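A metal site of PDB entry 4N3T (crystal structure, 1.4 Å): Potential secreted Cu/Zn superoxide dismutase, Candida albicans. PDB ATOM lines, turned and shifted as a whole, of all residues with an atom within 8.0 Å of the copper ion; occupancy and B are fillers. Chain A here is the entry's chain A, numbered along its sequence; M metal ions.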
ATOM      1  N   PRO A  51      -9.016  22.889  -1.575  1.00  0.00           N
ATOM      2  CA  PRO A  51      -7.735  23.254  -2.164  1.00  0.00           C
ATOM      3  C   PRO A  51      -6.666  23.416  -1.088  1.00  0.00           C
ATOM      4  O   PRO A  51      -6.955  23.795   0.045  1.00  0.00           O
ATOM      5  CB  PRO A  51      -8.036  24.602  -2.836  1.00  0.00           C
ATOM      6  CG  PRO A  51      -9.531  24.592  -3.074  1.00  0.00           C
ATOM      7  CD  PRO A  51     -10.094  23.844  -1.891  1.00  0.00           C
ATOM      8  N   TYR A  52      -5.433  23.096  -1.451  1.00  0.00           N
ATOM      9  CA  TYR A  52      -4.317  23.338  -0.557  1.00  0.00           C
ATOM     10  C   TYR A  52      -3.106  23.697  -1.379  1.00  0.00           C
ATOM     11  O   TYR A  52      -2.911  23.172  -2.490  1.00  0.00           O
ATOM     12  CB  TYR A  52      -4.069  22.156   0.376  1.00  0.00           C
ATOM     13  CG  TYR A  52      -3.593  20.880  -0.285  1.00  0.00           C
ATOM     14  CD1 TYR A  52      -4.460  20.086  -1.013  1.00  0.00           C
ATOM     15  CD2 TYR A  52      -2.272  20.456  -0.146  1.00  0.00           C
ATOM     16  CE1 TYR A  52      -4.035  18.903  -1.595  1.00  0.00           C
ATOM     17  CE2 TYR A  52      -1.828  19.276  -0.723  1.00  0.00           C
ATOM     18  CZ  TYR A  52      -2.709  18.503  -1.451  1.00  0.00           C
ATOM     19  OH  TYR A  52      -2.274  17.321  -2.031  1.00  0.00           O
ATOM     20  N   HIS A  53      -2.312  24.630  -0.861  1.00  0.00           N
ATOM     21  CA  HIS A  53      -1.195  25.161  -1.618  1.00  0.00           C
ATOM     22  C   HIS A  53      -0.041  25.476  -0.681  1.00  0.00           C
ATOM     23  O   HIS A  53      -0.237  25.714   0.516  1.00  0.00           O
ATOM     24  CB  HIS A  53      -1.583  26.453  -2.354  1.00  0.00           C
ATOM     25  CG  HIS A  53      -2.997  26.485  -2.831  1.00  0.00           C
ATOM     26  ND1 HIS A  53      -4.014  27.090  -2.121  1.00  0.00           N
ATOM     27  CD2 HIS A  53      -3.576  25.992  -3.956  1.00  0.00           C
ATOM     28  CE1 HIS A  53      -5.146  26.968  -2.779  1.00  0.00           C
ATOM     29  NE2 HIS A  53      -4.911  26.300  -3.895  1.00  0.00           N
ATOM     30  N   VAL A  54       1.159  25.514  -1.247  1.00  0.00           N
ATOM     31  CA  VAL A  54       2.289  26.116  -0.571  1.00  0.00           C
ATOM     32  C   VAL A  54       2.126  27.626  -0.724  1.00  0.00           C
ATOM     33  O   VAL A  54       1.900  28.120  -1.824  1.00  0.00           O
ATOM     34  CB  VAL A  54       3.614  25.688  -1.223  1.00  0.00           C
ATOM     35  CG1 VAL A  54       4.782  26.325  -0.481  1.00  0.00           C
ATOM     36  CG2 VAL A  54       3.735  24.186  -1.228  1.00  0.00           C
ATOM     37  N   HIS A  55       2.217  28.345   0.403  1.00  0.00           N
ATOM     38  CA  HIS A  55       2.132  29.801   0.384  1.00  0.00           C
ATOM     39  C   HIS A  55       3.496  30.419   0.634  1.00  0.00           C
ATOM     40  O   HIS A  55       4.438  29.723   1.029  1.00  0.00           O
ATOM     41  CB  HIS A  55       1.082  30.311   1.388  1.00  0.00           C
ATOM     42  CG  HIS A  55      -0.333  30.117   0.918  1.00  0.00           C
ATOM     43  ND1 HIS A  55      -1.201  31.166   0.734  1.00  0.00           N
ATOM     44  CD2 HIS A  55      -1.004  28.995   0.582  1.00  0.00           C
ATOM     45  CE1 HIS A  55      -2.362  30.698   0.300  1.00  0.00           C
ATOM     46  NE2 HIS A  55      -2.271  29.376   0.205  1.00  0.00           N
ATOM     47  N   CYS A  65      -3.839  32.328   9.299  1.00  0.00           N
ATOM     48  CA  CYS A  65      -3.557  31.765   7.982  1.00  0.00           C
ATOM     49  C   CYS A  65      -3.482  32.818   6.891  1.00  0.00           C
ATOM     50  O   CYS A  65      -2.880  32.590   5.860  1.00  0.00           O
ATOM     51  CB  CYS A  65      -4.587  30.698   7.641  1.00  0.00           C
ATOM     52  SG  CYS A  65      -4.585  29.291   8.773  1.00  0.00           S
ATOM     53  N   THR A  68       0.116  34.187   5.733  1.00  0.00           N
ATOM     54  CA  THR A  68       0.956  33.442   4.805  1.00  0.00           C
ATOM     55  C   THR A  68       0.926  34.066   3.410  1.00  0.00           C
ATOM     56  O   THR A  68       1.706  33.676   2.529  1.00  0.00           O
ATOM     57  CB  THR A  68       0.521  31.976   4.689  1.00  0.00           C
ATOM     58  OG1 THR A  68      -0.789  31.908   4.137  1.00  0.00           O
ATOM     59  CG2 THR A  68       0.539  31.292   6.054  1.00  0.00           C
ATOM     60  N   GLU A  69       0.026  35.026   3.210  1.00  0.00           N
ATOM     61  CA  GLU A  69      -0.121  35.739   1.941  1.00  0.00           C
ATOM     62  C   GLU A  69      -0.441  34.810   0.759  1.00  0.00           C
ATOM     63  O   GLU A  69      -1.267  33.911   0.889  1.00  0.00           O
ATOM     64  CB  GLU A  69       1.089  36.649   1.683  1.00  0.00           C
ATOM     65  CG  GLU A  69       1.291  37.667   2.810  1.00  0.00           C
ATOM     66  CD  GLU A  69       2.496  38.561   2.614  1.00  0.00           C
ATOM     67  OE1 GLU A  69       3.075  38.574   1.498  1.00  0.00           O
ATOM     68  OE2 GLU A  69       2.869  39.262   3.579  1.00  0.00           O
ATOM     69  N   ASN A  70       0.190  35.048  -0.392  1.00  0.00           N
ATOM     70  CA  ASN A  70      -0.217  34.361  -1.620  1.00  0.00           C
ATOM     71  C   ASN A  70       0.416  32.996  -1.843  1.00  0.00           C
ATOM     72  O   ASN A  70       1.240  32.541  -1.049  1.00  0.00           O
ATOM     73  CB  ASN A  70       0.056  35.253  -2.849  1.00  0.00           C
ATOM     74  CG  ASN A  70      -0.520  36.645  -2.697  1.00  0.00           C
ATOM     75  OD1 ASN A  70      -1.601  36.831  -2.145  1.00  0.00           O
ATOM     76  ND2 ASN A  70       0.214  37.642  -3.201  1.00  0.00           N
ATOM     77  N   HIS A  71       0.018  32.343  -2.938  1.00  0.00           N
ATOM     78  CA  HIS A  71       0.575  31.042  -3.311  1.00  0.00           C
ATOM     79  C   HIS A  71       2.021  31.202  -3.708  1.00  0.00           C
ATOM     80  O   HIS A  71       2.407  32.209  -4.296  1.00  0.00           O
ATOM     81  CB  HIS A  71      -0.174  30.426  -4.497  1.00  0.00           C
ATOM     82  CG  HIS A  71      -1.634  30.183  -4.254  1.00  0.00           C
ATOM     83  ND1 HIS A  71      -2.449  29.601  -5.196  1.00  0.00           N
ATOM     84  CD2 HIS A  71      -2.413  30.443  -3.181  1.00  0.00           C
ATOM     85  CE1 HIS A  71      -3.680  29.518  -4.714  1.00  0.00           C
ATOM     86  NE2 HIS A  71      -3.681  30.021  -3.491  1.00  0.00           N
ATOM     87  N   PHE A  72       2.842  30.202  -3.390  1.00  0.00           N
ATOM     88  CA  PHE A  72       4.215  30.177  -3.849  1.00  0.00           C
ATOM     89  C   PHE A  72       4.194  29.945  -5.367  1.00  0.00           C
ATOM     90  O   PHE A  72       3.771  28.887  -5.839  1.00  0.00           O
ATOM     91  CB  PHE A  72       4.975  29.066  -3.129  1.00  0.00           C
ATOM     92  CG  PHE A  72       6.403  28.917  -3.553  1.00  0.00           C
ATOM     93  CD1 PHE A  72       7.286  29.977  -3.470  1.00  0.00           C
ATOM     94  CD2 PHE A  72       6.861  27.702  -4.043  1.00  0.00           C
ATOM     95  CE1 PHE A  72       8.608  29.825  -3.853  1.00  0.00           C
ATOM     96  CE2 PHE A  72       8.173  27.542  -4.420  1.00  0.00           C
ATOM     97  CZ  PHE A  72       9.045  28.594  -4.331  1.00  0.00           C
ATOM     98  N   GLU A  88       0.831  26.908 -10.743  1.00  0.00           N
ATOM     99  CA  GLU A  88       1.845  27.434  -9.832  1.00  0.00           C
ATOM    100  C   GLU A  88       2.553  26.271  -9.155  1.00  0.00           C
ATOM    101  O   GLU A  88       1.944  25.236  -8.876  1.00  0.00           O
ATOM    102  CB  GLU A  88       1.193  28.309  -8.764  1.00  0.00           C
ATOM    103  CG  GLU A  88       0.226  29.337  -9.293  1.00  0.00           C
ATOM    104  CD  GLU A  88      -0.659  29.903  -8.201  1.00  0.00           C
ATOM    105  OE1 GLU A  88      -0.819  31.134  -8.140  1.00  0.00           O
ATOM    106  OE2 GLU A  88      -1.195  29.095  -7.405  1.00  0.00           O
ATOM    107  N   GLY A  90       3.454  25.979  -6.139  1.00  0.00           N
ATOM    108  CA  GLY A  90       2.802  25.692  -4.879  1.00  0.00           C
ATOM    109  C   GLY A  90       1.394  25.140  -4.982  1.00  0.00           C
ATOM    110  O   GLY A  90       0.818  24.755  -3.958  1.00  0.00           O
ATOM    111  N   ASP A  91       0.838  25.085  -6.186  1.00  0.00           N
ATOM    112  CA  ASP A  91      -0.554  24.651  -6.353  1.00  0.00           C
ATOM    113  C   ASP A  91      -0.674  23.128  -6.386  1.00  0.00           C
ATOM    114  O   ASP A  91      -0.970  22.528  -7.429  1.00  0.00           O
ATOM    115  CB  ASP A  91      -1.181  25.295  -7.597  1.00  0.00           C
ATOM    116  CG  ASP A  91      -2.666  24.987  -7.742  1.00  0.00           C
ATOM    117  OD1 ASP A  91      -3.267  24.476  -6.770  1.00  0.00           O
ATOM    118  OD2 ASP A  91      -3.225  25.261  -8.823  1.00  0.00           O
ATOM    119  N   SER A 127       4.940  27.676   3.922  1.00  0.00           N
ATOM    120  CA  SER A 127       3.782  27.170   4.654  1.00  0.00           C
ATOM    121  C   SER A 127       2.821  26.475   3.710  1.00  0.00           C
ATOM    122  O   SER A 127       2.917  26.616   2.497  1.00  0.00           O
ATOM    123  CB  SER A 127       3.047  28.338   5.336  1.00  0.00           C
ATOM    124  OG  SER A 127       2.625  29.297   4.384  1.00  0.00           O
ATOM    125  N   ILE A 128       1.905  25.707   4.292  1.00  0.00           N
ATOM    126  CA  ILE A 128       0.803  25.146   3.526  1.00  0.00           C
ATOM    127  C   ILE A 128      -0.492  25.610   4.159  1.00  0.00           C
ATOM    128  O   ILE A 128      -0.632  25.634   5.379  1.00  0.00           O
ATOM    129  CB  ILE A 128       0.855  23.614   3.490  1.00  0.00           C
ATOM    130  CG1 ILE A 128       2.152  23.161   2.841  1.00  0.00           C
ATOM    131  CG2 ILE A 128      -0.343  23.049   2.731  1.00  0.00           C
ATOM    132  CD1 ILE A 128       2.374  21.682   2.878  1.00  0.00           C
ATOM    133  N   VAL A 129      -1.441  26.010   3.321  1.00  0.00           N
ATOM    134  CA  VAL A 129      -2.757  26.420   3.768  1.00  0.00           C
ATOM    135  C   VAL A 129      -3.783  25.483   3.138  1.00  0.00           C
ATOM    136  O   VAL A 129      -3.691  25.162   1.954  1.00  0.00           O
ATOM    137  CB  VAL A 129      -3.078  27.871   3.356  1.00  0.00           C
ATOM    138  CG1 VAL A 129      -4.493  28.246   3.801  1.00  0.00           C
ATOM    139  CG2 VAL A 129      -2.058  28.842   3.947  1.00  0.00           C
ATOM    140  N   ILE A 130      -4.739  25.029   3.947  1.00  0.00           N
ATOM    141  CA  ILE A 130      -5.870  24.260   3.463  1.00  0.00           C
ATOM    142  C   ILE A 130      -7.088  25.180   3.478  1.00  0.00           C
ATOM    143  O   ILE A 130      -7.342  25.853   4.473  1.00  0.00           O
ATOM    144  CB  ILE A 130      -6.151  23.031   4.355  1.00  0.00           C
ATOM    145  CG1 ILE A 130      -4.939  22.107   4.361  1.00  0.00           C
ATOM    146  CG2 ILE A 130      -7.422  22.274   3.906  1.00  0.00           C
ATOM    147  CD1 ILE A 130      -5.000  21.006   5.397  1.00  0.00           C
ATOM    148  N   HIS A 131      -7.811  25.211   2.355  1.00  0.00           N
ATOM    149  CA  HIS A 131      -8.955  26.094   2.175  1.00  0.00           C
ATOM    150  C   HIS A 131     -10.260  25.335   2.070  1.00  0.00           C
ATOM    151  O   HIS A 131     -10.287  24.201   1.597  1.00  0.00           O
ATOM    152  CB  HIS A 131      -8.828  26.868   0.869  1.00  0.00           C
ATOM    153  CG  HIS A 131      -7.580  27.666   0.736  1.00  0.00           C
ATOM    154  ND1 HIS A 131      -7.569  29.038   0.771  1.00  0.00           N
ATOM    155  CD2 HIS A 131      -6.298  27.287   0.498  1.00  0.00           C
ATOM    156  CE1 HIS A 131      -6.335  29.474   0.599  1.00  0.00           C
ATOM    157  NE2 HIS A 131      -5.546  28.433   0.424  1.00  0.00           N
ATOM    158  N   GLY A 135     -12.696  29.163  -0.657  1.00  0.00           N
ATOM    159  CA  GLY A 135     -11.454  29.891  -0.498  1.00  0.00           C
ATOM    160  C   GLY A 135     -11.085  30.255   0.933  1.00  0.00           C
ATOM    161  O   GLY A 135      -9.938  30.614   1.194  1.00  0.00           O
ATOM    162  N   THR A 136     -12.045  30.167   1.842  1.00  0.00           N
ATOM    163  CA  THR A 136     -11.785  30.468   3.250  1.00  0.00           C
ATOM    164  C   THR A 136     -10.620  29.626   3.776  1.00  0.00           C
ATOM    165  O   THR A 136     -10.577  28.415   3.553  1.00  0.00           O
ATOM    166  CB  THR A 136     -13.019  30.201   4.129  1.00  0.00           C
ATOM    167  OG1 THR A 136     -14.108  31.020   3.685  1.00  0.00           O
ATOM    168  CG2 THR A 136     -12.715  30.520   5.593  1.00  0.00           C
ATOM    169  N   ARG A 137      -9.667  30.259   4.458  1.00  0.00           N
ATOM    170  CA  ARG A 137      -8.541  29.514   4.983  1.00  0.00           C
ATOM    171  C   ARG A 137      -8.928  28.830   6.285  1.00  0.00           C
ATOM    172  O   ARG A 137      -9.386  29.481   7.234  1.00  0.00           O
ATOM    173  CB  ARG A 137      -7.330  30.445   5.151  1.00  0.00           C
ATOM    174  CG  ARG A 137      -6.970  31.155   3.850  1.00  0.00           C
ATOM    175  CD  ARG A 137      -5.708  32.018   3.921  1.00  0.00           C
ATOM    176  NE  ARG A 137      -5.449  32.610   2.610  1.00  0.00           N
ATOM    177  CZ  ARG A 137      -4.289  33.113   2.204  1.00  0.00           C
ATOM    178  NH1 ARG A 137      -3.238  33.119   3.003  1.00  0.00           N
ATOM    179  NH2 ARG A 137      -4.192  33.635   0.991  1.00  0.00           N
ATOM    180  N   ASN A 139      -7.008  25.933   7.966  1.00  0.00           N
ATOM    181  CA  ASN A 139      -5.857  25.672   8.819  1.00  0.00           C
ATOM    182  C   ASN A 139      -4.579  25.803   7.989  1.00  0.00           C
ATOM    183  O   ASN A 139      -4.618  25.817   6.741  1.00  0.00           O
ATOM    184  CB  ASN A 139      -5.983  24.293   9.489  1.00  0.00           C
ATOM    185  CG  ASN A 139      -5.181  24.170  10.770  1.00  0.00           C
ATOM    186  OD1 ASN A 139      -4.365  25.040  11.103  1.00  0.00           O
ATOM    187  ND2 ASN A 139      -5.400  23.078  11.497  1.00  0.00           N
HETATM  188 CU    CU M   1      -3.763  28.297  -0.472  1.00  0.00          CU
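O of Glu 69 is in hydrogen-bond range of ND1 of His 55, 2.8 Å away.
A ring nitrogen (ND1) of His 55 lies close to the backbone carbonyl oxygen (O) of Asn 70.
The backbone NH of His 55 is in hydrogen-bond range of the backbone carbonyl oxygen of Ser 127, 2.8 Å away.
N of His 131 lies within hydrogen-bond range of O of Pro 51 (2.8 Å).
The backbone carbonyl oxygen (O) of Gly 135 is in hydrogen-bond range of a ring nitrogen (ND1) of His 131, at 2.9 Å.
A ring nitrogen (NE2) of His 71 sits close to a ring nitrogen (ND1) of His 53, 3.3 Å away.
The backbone carbonyl oxygen of His 53 is in hydrogen-bond range of the backbone NH of Val 129, 3.1 Å away.
A ring nitrogen (ND1) of His 71 is in hydrogen-bond range of the side-chain carboxylate of Glu 88, at 2.6 Å.
Merely in contact with the copper ion: His 71 (3.5 Å) and Val 129 (3.9 Å).
Five residues have an atom within 4 Å of the copper ion: His 53, His 55, His 71, Val 129 and His 131.
The nearest printed residue that does not touch the copper ion is Tyr 52 (4.7 Å).
The copper ion is bound by NE2 of His 55 (2.0 Å), NE2 of His 131 (2.0 Å) and ND1 of His 53 (2.1 Å).
The copper ion has three donor atoms within binding distance.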
